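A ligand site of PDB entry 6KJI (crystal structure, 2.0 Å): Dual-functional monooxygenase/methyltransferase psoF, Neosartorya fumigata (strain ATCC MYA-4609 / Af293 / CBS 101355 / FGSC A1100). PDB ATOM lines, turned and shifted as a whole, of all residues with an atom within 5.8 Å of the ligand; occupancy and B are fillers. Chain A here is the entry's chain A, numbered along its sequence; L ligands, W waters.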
ATOM      1  N   TYR A 151     -24.685   6.037  12.571  1.00  0.00           N
ATOM      2  CA  TYR A 151     -23.548   5.387  13.199  1.00  0.00           C
ATOM      3  C   TYR A 151     -22.795   6.405  14.051  1.00  0.00           C
ATOM      4  O   TYR A 151     -22.233   6.069  15.097  1.00  0.00           O
ATOM      5  CB  TYR A 151     -22.603   4.823  12.124  1.00  0.00           C
ATOM      6  CG  TYR A 151     -23.250   3.860  11.141  1.00  0.00           C
ATOM      7  CD1 TYR A 151     -24.207   2.941  11.542  1.00  0.00           C
ATOM      8  CD2 TYR A 151     -22.891   3.897   9.799  1.00  0.00           C
ATOM      9  CE1 TYR A 151     -24.793   2.072  10.618  1.00  0.00           C
ATOM     10  CE2 TYR A 151     -23.460   3.030   8.884  1.00  0.00           C
ATOM     11  CZ  TYR A 151     -24.408   2.131   9.286  1.00  0.00           C
ATOM     12  OH  TYR A 151     -24.966   1.279   8.350  1.00  0.00           O
ATOM     13  N   LEU A 152     -22.841   7.663  13.622  1.00  0.00           N
ATOM     14  CA  LEU A 152     -22.203   8.792  14.314  1.00  0.00           C
ATOM     15  C   LEU A 152     -23.068   9.312  15.437  1.00  0.00           C
ATOM     16  O   LEU A 152     -22.634  10.145  16.231  1.00  0.00           O
ATOM     17  CB  LEU A 152     -21.900   9.918  13.327  1.00  0.00           C
ATOM     18  CG  LEU A 152     -20.979   9.540  12.164  1.00  0.00           C
ATOM     19  CD1 LEU A 152     -20.664  10.743  11.283  1.00  0.00           C
ATOM     20  CD2 LEU A 152     -19.699   8.898  12.683  1.00  0.00           C
ATOM     21  N   ASN A 160     -18.262   3.251  20.713  1.00  0.00           N
ATOM     22  CA  ASN A 160     -17.116   3.589  19.864  1.00  0.00           C
ATOM     23  C   ASN A 160     -15.996   4.248  20.664  1.00  0.00           C
ATOM     24  O   ASN A 160     -14.815   4.033  20.383  1.00  0.00           O
ATOM     25  CB  ASN A 160     -17.552   4.515  18.723  1.00  0.00           C
ATOM     26  CG  ASN A 160     -18.153   3.765  17.565  1.00  0.00           C
ATOM     27  OD1 ASN A 160     -17.790   2.630  17.289  1.00  0.00           O
ATOM     28  ND2 ASN A 160     -19.087   4.420  16.867  1.00  0.00           N
ATOM     29  N   GLU A 181      -9.257  -3.349  10.944  1.00  0.00           N
ATOM     30  CA  GLU A 181     -10.649  -3.060  11.234  1.00  0.00           C
ATOM     31  C   GLU A 181     -11.531  -3.749  10.189  1.00  0.00           C
ATOM     32  O   GLU A 181     -11.323  -3.633   8.974  1.00  0.00           O
ATOM     33  CB  GLU A 181     -10.919  -1.556  11.309  1.00  0.00           C
ATOM     34  CG  GLU A 181     -12.381  -1.245  11.718  1.00  0.00           C
ATOM     35  CD  GLU A 181     -12.679   0.226  11.906  1.00  0.00           C
ATOM     36  OE1 GLU A 181     -11.761   1.077  11.763  1.00  0.00           O
ATOM     37  OE2 GLU A 181     -13.857   0.533  12.224  1.00  0.00           O
ATOM     38  N   ILE A 182     -12.487  -4.507  10.703  1.00  0.00           N
ATOM     39  CA  ILE A 182     -13.478  -5.203   9.906  1.00  0.00           C
ATOM     40  C   ILE A 182     -14.703  -4.325   9.812  1.00  0.00           C
ATOM     41  O   ILE A 182     -15.078  -3.667  10.787  1.00  0.00           O
ATOM     42  CB  ILE A 182     -13.858  -6.559  10.525  1.00  0.00           C
ATOM     43  CG1 ILE A 182     -12.634  -7.437  10.702  1.00  0.00           C
ATOM     44  CG2 ILE A 182     -14.901  -7.258   9.661  1.00  0.00           C
ATOM     45  CD1 ILE A 182     -12.924  -8.744  11.458  1.00  0.00           C
ATOM     46  N   GLY A 183     -15.346  -4.324   8.641  1.00  0.00           N
ATOM     47  CA  GLY A 183     -16.537  -3.529   8.422  1.00  0.00           C
ATOM     48  C   GLY A 183     -16.391  -2.082   8.850  1.00  0.00           C
ATOM     49  O   GLY A 183     -17.272  -1.504   9.491  1.00  0.00           O
ATOM     50  N   ALA A 184     -15.272  -1.465   8.461  1.00  0.00           N
ATOM     51  CA  ALA A 184     -14.987  -0.093   8.861  1.00  0.00           C
ATOM     52  C   ALA A 184     -16.005   0.877   8.255  1.00  0.00           C
ATOM     53  O   ALA A 184     -16.237   1.957   8.794  1.00  0.00           O
ATOM     54  CB  ALA A 184     -13.565   0.302   8.464  1.00  0.00           C
ATOM     55  N   GLY A 185     -16.624   0.471   7.150  1.00  0.00           N
ATOM     56  CA  GLY A 185     -17.619   1.302   6.487  1.00  0.00           C
ATOM     57  C   GLY A 185     -17.070   2.675   6.135  1.00  0.00           C
ATOM     58  O   GLY A 185     -16.000   2.783   5.554  1.00  0.00           O
ATOM     59  N   THR A 186     -17.803   3.720   6.523  1.00  0.00           N
ATOM     60  CA  THR A 186     -17.398   5.095   6.238  1.00  0.00           C
ATOM     61  C   THR A 186     -16.431   5.626   7.282  1.00  0.00           C
ATOM     62  O   THR A 186     -16.042   6.783   7.239  1.00  0.00           O
ATOM     63  CB  THR A 186     -18.605   6.048   6.159  1.00  0.00           C
ATOM     64  OG1 THR A 186     -19.301   6.048   7.418  1.00  0.00           O
ATOM     65  CG2 THR A 186     -19.559   5.646   5.052  1.00  0.00           C
ATOM     66  N   GLY A 187     -16.046   4.780   8.238  1.00  0.00           N
ATOM     67  CA  GLY A 187     -15.000   5.127   9.176  1.00  0.00           C
ATOM     68  C   GLY A 187     -15.445   5.828  10.444  1.00  0.00           C
ATOM     69  O   GLY A 187     -14.685   6.580  11.049  1.00  0.00           O
ATOM     70  N   GLY A 188     -16.697   5.590  10.841  1.00  0.00           N
ATOM     71  CA  GLY A 188     -17.209   6.170  12.066  1.00  0.00           C
ATOM     72  C   GLY A 188     -16.449   5.738  13.306  1.00  0.00           C
ATOM     73  O   GLY A 188     -16.078   6.556  14.150  1.00  0.00           O
ATOM     74  N   THR A 189     -16.230   4.433  13.446  1.00  0.00           N
ATOM     75  CA  THR A 189     -15.450   3.953  14.579  1.00  0.00           C
ATOM     76  C   THR A 189     -13.989   4.366  14.393  1.00  0.00           C
ATOM     77  O   THR A 189     -13.352   4.835  15.336  1.00  0.00           O
ATOM     78  CB  THR A 189     -15.549   2.436  14.762  1.00  0.00           C
ATOM     79  OG1 THR A 189     -16.924   2.067  14.893  1.00  0.00           O
ATOM     80  CG2 THR A 189     -14.800   1.998  16.021  1.00  0.00           C
ATOM     81  N   ASP A 212     -13.419  -3.371   4.507  1.00  0.00           N
ATOM     82  CA  ASP A 212     -14.861  -3.494   4.494  1.00  0.00           C
ATOM     83  C   ASP A 212     -15.243  -4.542   3.466  1.00  0.00           C
ATOM     84  O   ASP A 212     -14.410  -4.937   2.638  1.00  0.00           O
ATOM     85  CB  ASP A 212     -15.542  -2.158   4.185  1.00  0.00           C
ATOM     86  CG  ASP A 212     -17.020  -2.150   4.571  1.00  0.00           C
ATOM     87  OD1 ASP A 212     -17.870  -2.616   3.773  1.00  0.00           O
ATOM     88  OD2 ASP A 212     -17.329  -1.669   5.682  1.00  0.00           O
ATOM     89  N   LEU A 213     -16.473  -5.013   3.544  1.00  0.00           N
ATOM     90  CA  LEU A 213     -16.998  -5.909   2.520  1.00  0.00           C
ATOM     91  C   LEU A 213     -16.938  -5.227   1.145  1.00  0.00           C
ATOM     92  O   LEU A 213     -16.605  -5.850   0.136  1.00  0.00           O
ATOM     93  CB  LEU A 213     -18.446  -6.266   2.854  1.00  0.00           C
ATOM     94  CG  LEU A 213     -19.215  -7.062   1.812  1.00  0.00           C
ATOM     95  CD1 LEU A 213     -18.596  -8.447   1.615  1.00  0.00           C
ATOM     96  CD2 LEU A 213     -20.674  -7.143   2.221  1.00  0.00           C
ATOM     97  N   SER A 214     -17.244  -3.937   1.138  1.00  0.00           N
ATOM     98  CA  SER A 214     -17.354  -3.182  -0.096  1.00  0.00           C
ATOM     99  C   SER A 214     -16.296  -2.107  -0.178  1.00  0.00           C
ATOM    100  O   SER A 214     -16.196  -1.256   0.708  1.00  0.00           O
ATOM    101  CB  SER A 214     -18.738  -2.537  -0.199  1.00  0.00           C
ATOM    102  OG  SER A 214     -18.827  -1.660  -1.308  1.00  0.00           O
ATOM    103  N   PHE A 217     -16.669   2.122  -0.017  1.00  0.00           N
ATOM    104  CA  PHE A 217     -16.496   3.039   1.111  1.00  0.00           C
ATOM    105  C   PHE A 217     -15.128   3.686   1.106  1.00  0.00           C
ATOM    106  O   PHE A 217     -14.943   4.743   1.711  1.00  0.00           O
ATOM    107  CB  PHE A 217     -16.702   2.303   2.447  1.00  0.00           C
ATOM    108  CG  PHE A 217     -18.101   1.860   2.691  1.00  0.00           C
ATOM    109  CD1 PHE A 217     -19.075   2.762   3.080  1.00  0.00           C
ATOM    110  CD2 PHE A 217     -18.458   0.533   2.547  1.00  0.00           C
ATOM    111  CE1 PHE A 217     -20.370   2.344   3.320  1.00  0.00           C
ATOM    112  CE2 PHE A 217     -19.748   0.112   2.779  1.00  0.00           C
ATOM    113  CZ  PHE A 217     -20.708   1.023   3.162  1.00  0.00           C
ATOM    114  N   LEU A 237     -12.417  -6.943   2.556  1.00  0.00           N
ATOM    115  CA  LEU A 237     -12.454  -8.118   3.394  1.00  0.00           C
ATOM    116  C   LEU A 237     -13.901  -8.494   3.650  1.00  0.00           C
ATOM    117  O   LEU A 237     -14.662  -7.735   4.255  1.00  0.00           O
ATOM    118  CB  LEU A 237     -11.708  -7.892   4.710  1.00  0.00           C
ATOM    119  CG  LEU A 237     -11.861  -9.015   5.739  1.00  0.00           C
ATOM    120  CD1 LEU A 237     -11.414 -10.373   5.155  1.00  0.00           C
ATOM    121  CD2 LEU A 237     -11.063  -8.675   6.984  1.00  0.00           C
ATOM    122  N   ASN A 238     -14.279  -9.654   3.135  1.00  0.00           N
ATOM    123  CA  ASN A 238     -15.534 -10.285   3.482  1.00  0.00           C
ATOM    124  C   ASN A 238     -15.232 -11.276   4.584  1.00  0.00           C
ATOM    125  O   ASN A 238     -14.641 -12.331   4.341  1.00  0.00           O
ATOM    126  CB  ASN A 238     -16.146 -10.969   2.252  1.00  0.00           C
ATOM    127  CG  ASN A 238     -17.471 -11.626   2.563  1.00  0.00           C
ATOM    128  OD1 ASN A 238     -17.799 -11.883   3.730  1.00  0.00           O
ATOM    129  ND2 ASN A 238     -18.248 -11.905   1.530  1.00  0.00           N
ATOM    130  N   ILE A 239     -15.620 -10.927   5.814  1.00  0.00           N
ATOM    131  CA  ILE A 239     -15.232 -11.713   6.973  1.00  0.00           C
ATOM    132  C   ILE A 239     -15.957 -13.062   7.007  1.00  0.00           C
ATOM    133  O   ILE A 239     -15.628 -13.933   7.804  1.00  0.00           O
ATOM    134  CB  ILE A 239     -15.458 -10.927   8.291  1.00  0.00           C
ATOM    135  CG1 ILE A 239     -14.693 -11.563   9.457  1.00  0.00           C
ATOM    136  CG2 ILE A 239     -16.948 -10.765   8.591  1.00  0.00           C
ATOM    137  CD1 ILE A 239     -13.201 -11.672   9.204  1.00  0.00           C
ATOM    138  N   GLU A 240     -16.923 -13.244   6.122  1.00  0.00           N
ATOM    139  CA  GLU A 240     -17.592 -14.535   6.031  1.00  0.00           C
ATOM    140  C   GLU A 240     -16.719 -15.543   5.274  1.00  0.00           C
ATOM    141  O   GLU A 240     -16.958 -16.755   5.326  1.00  0.00           O
ATOM    142  CB  GLU A 240     -18.960 -14.397   5.367  1.00  0.00           C
ATOM    143  CG  GLU A 240     -19.872 -13.406   6.093  1.00  0.00           C
ATOM    144  CD  GLU A 240     -21.354 -13.680   5.832  1.00  0.00           C
ATOM    145  OE1 GLU A 240     -21.798 -14.800   6.143  1.00  0.00           O
ATOM    146  OE2 GLU A 240     -22.076 -12.767   5.385  1.00  0.00           O
ATOM    147  N   ALA A 258     -14.022  -4.489  15.339  1.00  0.00           N
ATOM    148  CA  ALA A 258     -15.223  -4.855  14.590  1.00  0.00           C
ATOM    149  C   ALA A 258     -16.431  -4.217  15.244  1.00  0.00           C
ATOM    150  O   ALA A 258     -16.971  -4.717  16.217  1.00  0.00           O
ATOM    151  CB  ALA A 258     -15.375  -6.349  14.519  1.00  0.00           C
ATOM    152  N   ALA A 259     -16.827  -3.056  14.736  1.00  0.00           N
ATOM    153  CA  ALA A 259     -17.911  -2.303  15.338  1.00  0.00           C
ATOM    154  C   ALA A 259     -19.166  -2.439  14.505  1.00  0.00           C
ATOM    155  O   ALA A 259     -19.197  -2.009  13.348  1.00  0.00           O
ATOM    156  CB  ALA A 259     -17.513  -0.836  15.469  1.00  0.00           C
ATOM    157  N   ASN A 260     -20.188  -3.039  15.105  1.00  0.00           N
ATOM    158  CA  ASN A 260     -21.497  -3.113  14.474  1.00  0.00           C
ATOM    159  C   ASN A 260     -21.478  -3.845  13.123  1.00  0.00           C
ATOM    160  O   ASN A 260     -22.186  -3.476  12.184  1.00  0.00           O
ATOM    161  CB  ASN A 260     -22.060  -1.700  14.289  1.00  0.00           C
ATOM    162  CG  ASN A 260     -22.005  -0.883  15.577  1.00  0.00           C
ATOM    163  OD1 ASN A 260     -21.397   0.175  15.634  1.00  0.00           O
ATOM    164  ND2 ASN A 260     -22.659  -1.390  16.627  1.00  0.00           N
ATOM    165  N   VAL A 261     -20.669  -4.896  13.024  1.00  0.00           N
ATOM    166  CA  VAL A 261     -20.530  -5.621  11.767  1.00  0.00           C
ATOM    167  C   VAL A 261     -20.661  -7.142  11.885  1.00  0.00           C
ATOM    168  O   VAL A 261     -21.175  -7.784  10.979  1.00  0.00           O
ATOM    169  CB  VAL A 261     -19.178  -5.304  11.085  1.00  0.00           C
ATOM    170  CG1 VAL A 261     -18.017  -5.358  12.093  1.00  0.00           C
ATOM    171  CG2 VAL A 261     -18.948  -6.231   9.904  1.00  0.00           C
ATOM    172  N   ALA A 264     -23.861  -8.874  11.327  1.00  0.00           N
ATOM    173  CA  ALA A 264     -24.396  -8.758   9.973  1.00  0.00           C
ATOM    174  C   ALA A 264     -23.873  -9.872   9.056  1.00  0.00           C
ATOM    175  O   ALA A 264     -23.944  -9.773   7.845  1.00  0.00           O
ATOM    176  CB  ALA A 264     -24.050  -7.381   9.388  1.00  0.00           C
ATOM    177  N   THR A 265     -23.327 -10.926   9.650  1.00  0.00           N
ATOM    178  CA  THR A 265     -22.855 -12.076   8.869  1.00  0.00           C
ATOM    179  C   THR A 265     -23.792 -13.264   9.019  1.00  0.00           C
ATOM    180  O   THR A 265     -24.614 -13.295   9.921  1.00  0.00           O
ATOM    181  CB  THR A 265     -21.429 -12.464   9.275  1.00  0.00           C
ATOM    182  OG1 THR A 265     -21.419 -12.804  10.671  1.00  0.00           O
ATOM    183  CG2 THR A 265     -20.482 -11.310   9.032  1.00  0.00           C
HETATM  184  N1  LIG L   1     -18.015   0.057  11.690  1.00  0.00           N
HETATM  185  C1  LIG L   1     -18.755   1.249  11.289  1.00  0.00           C
HETATM  186  C2  LIG L   1     -19.842   0.888  10.283  1.00  0.00           C
HETATM  187  C3  LIG L   1     -20.780  -0.218  10.723  1.00  0.00           C
HETATM  188  S1  LIG L   1     -22.035  -0.586   9.448  1.00  0.00           S
HETATM  189  C4  LIG L   1     -19.358   1.956  12.508  1.00  0.00           C
HETATM  190  O1  LIG L   1     -19.558   1.359  13.570  1.00  0.00           O
HETATM  191  O2  LIG L   1     -19.663   3.142  12.457  1.00  0.00           O
HETATM  192  C5  LIG L   1     -21.464  -2.268   9.123  1.00  0.00           C
HETATM  193  C6  LIG L   1     -20.347  -2.344   8.092  1.00  0.00           C
HETATM  194  O3  LIG L   1     -19.983  -3.700   8.010  1.00  0.00           O
HETATM  195  C7  LIG L   1     -20.754  -1.907   6.682  1.00  0.00           C
HETATM  196  O4  LIG L   1     -19.831  -0.965   6.157  1.00  0.00           O
HETATM  197  C8  LIG L   1     -20.757  -3.170   5.858  1.00  0.00           C
HETATM  198  O5  LIG L   1     -20.323  -2.990   4.523  1.00  0.00           O
HETATM  199  C9  LIG L   1     -19.800  -4.049   6.655  1.00  0.00           C
HETATM  200  N2  LIG L   1     -20.058  -5.467   6.415  1.00  0.00           N
HETATM  201  C10 LIG L   1     -21.256  -6.103   6.245  1.00  0.00           C
HETATM  202  N3  LIG L   1     -21.006  -7.403   6.030  1.00  0.00           N
HETATM  203  C11 LIG L   1     -19.676  -7.603   6.051  1.00  0.00           C
HETATM  204  C12 LIG L   1     -18.891  -8.740   5.888  1.00  0.00           C
HETATM  205  N4  LIG L   1     -19.453  -9.916   5.651  1.00  0.00           N
HETATM  206  N5  LIG L   1     -17.530  -8.629   5.963  1.00  0.00           N
HETATM  207  C13 LIG L   1     -16.941  -7.412   6.206  1.00  0.00           C
HETATM  208  N6  LIG L   1     -17.718  -6.293   6.379  1.00  0.00           N
HETATM  209  C14 LIG L   1     -19.065  -6.396   6.298  1.00  0.00           C
HETATM  210  O   HOH W   1     -21.090   1.266   6.575  1.00  0.00           O
HETATM  211  O   HOH W   2     -15.567   2.355  11.350  1.00  0.00           O
HETATM  212  O   HOH W   3     -22.009  -3.030   2.358  1.00  0.00           O
HETATM  213  O   HOH W   4     -19.193   4.389   9.844  1.00  0.00           O
HETATM  214  O   HOH W   5     -14.223  -5.814   6.377  1.00  0.00           O
HETATM  215  O   HOH W   6     -15.623  -1.680  12.535  1.00  0.00           O
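Water W4 lies within hydrogen-bond range of an oxygen (O2) of the ligand (2.9 Å), the side-chain hydroxyl (OG1) of Thr 186 (2.9 Å) and the backbone NH (N) of Gly 188 (2.9 Å). Water W5 lies within hydrogen-bond range of O of Leu 237, N of Gly 183 and N of Asp 212. Water W2 lies within hydrogen-bond range of OE2 of Glu 181, O of Ala 184, N of Thr 189, N1 of the ligand and N of Gly 188.
A nitrogen (N5) of the ligand lies close to the backbone carbonyl oxygen (O) of Leu 237, 3.5 Å away. O of Ala 184 touches C1 of the ligand, 3.6 Å away. Gly 185 touches the ligand. Gly 188 touches the ligand. CE2 of Phe 217 touches O4 of the ligand, at 3.5 Å. Glu 240 touches the ligand (CG to N4, 3.5 Å). Val 261 touches the ligand (CG2 to O3, 3.3 Å). Thr 265 touches the ligand. 17 residues have an atom within 4 Å of the ligand: Tyr 151, Gly 183, Ala 184, Gly 185, Gly 188, Thr 189, Asp 212, Leu 213, Phe 217, Leu 237, Asn 238, Ile 239, Glu 240, Ala 259, Asn 260, Val 261 and Thr 265.
A nitrogen (N4) of the ligand lies within hydrogen-bond range of the side-chain amide oxygen (OD1) of Asn 238, at 3.2 Å. The side-chain hydroxyl (OH) of Tyr 151 sits close to a sulfur (S1) of the ligand (3.6 Å). The backbone carbonyl oxygen of Ala 259 is in hydrogen-bond range of a nitrogen (N1) of the ligand. N5 of the ligand sits at hydrogen-bond distance from N of Ile 239 (3.0 Å). N of Leu 213 sits at hydrogen-bond distance from N6 of the ligand, at 3.4 Å. OG1 of Thr 189 sits at hydrogen-bond distance from O1 of the ligand (3.0 Å). The side-chain amide oxygen of Asn 260 lies close to an oxygen (O1) of the ligand (3.0 Å). O5 of the ligand sits at hydrogen-bond distance from OD1 of Asp 212, at 2.6 Å. O of Gly 183 is in hydrogen-bond range of N1 of the ligand, at 2.8 Å.
OD1 of Asn 160 is in hydrogen-bond range of OG1 of Thr 189, at 2.6 Å. O of Asp 212 lies within hydrogen-bond range of N of Leu 237 (2.8 Å). OD2 of Asp 212 lies within hydrogen-bond range of N of Ala 184. The side-chain carboxylate of Asp 212 is in hydrogen-bond range of the backbone NH of Gly 185 (2.7 Å). The backbone NH (N) of Ser 214 sits at hydrogen-bond distance from the side-chain carboxylate (OD1) of Asp 212 (3.0 Å). O of Leu 237 sits at hydrogen-bond distance from N of Leu 213 (3.3 Å). N of Glu 240 lies within hydrogen-bond range of OD1 of Asn 238 (2.9 Å).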
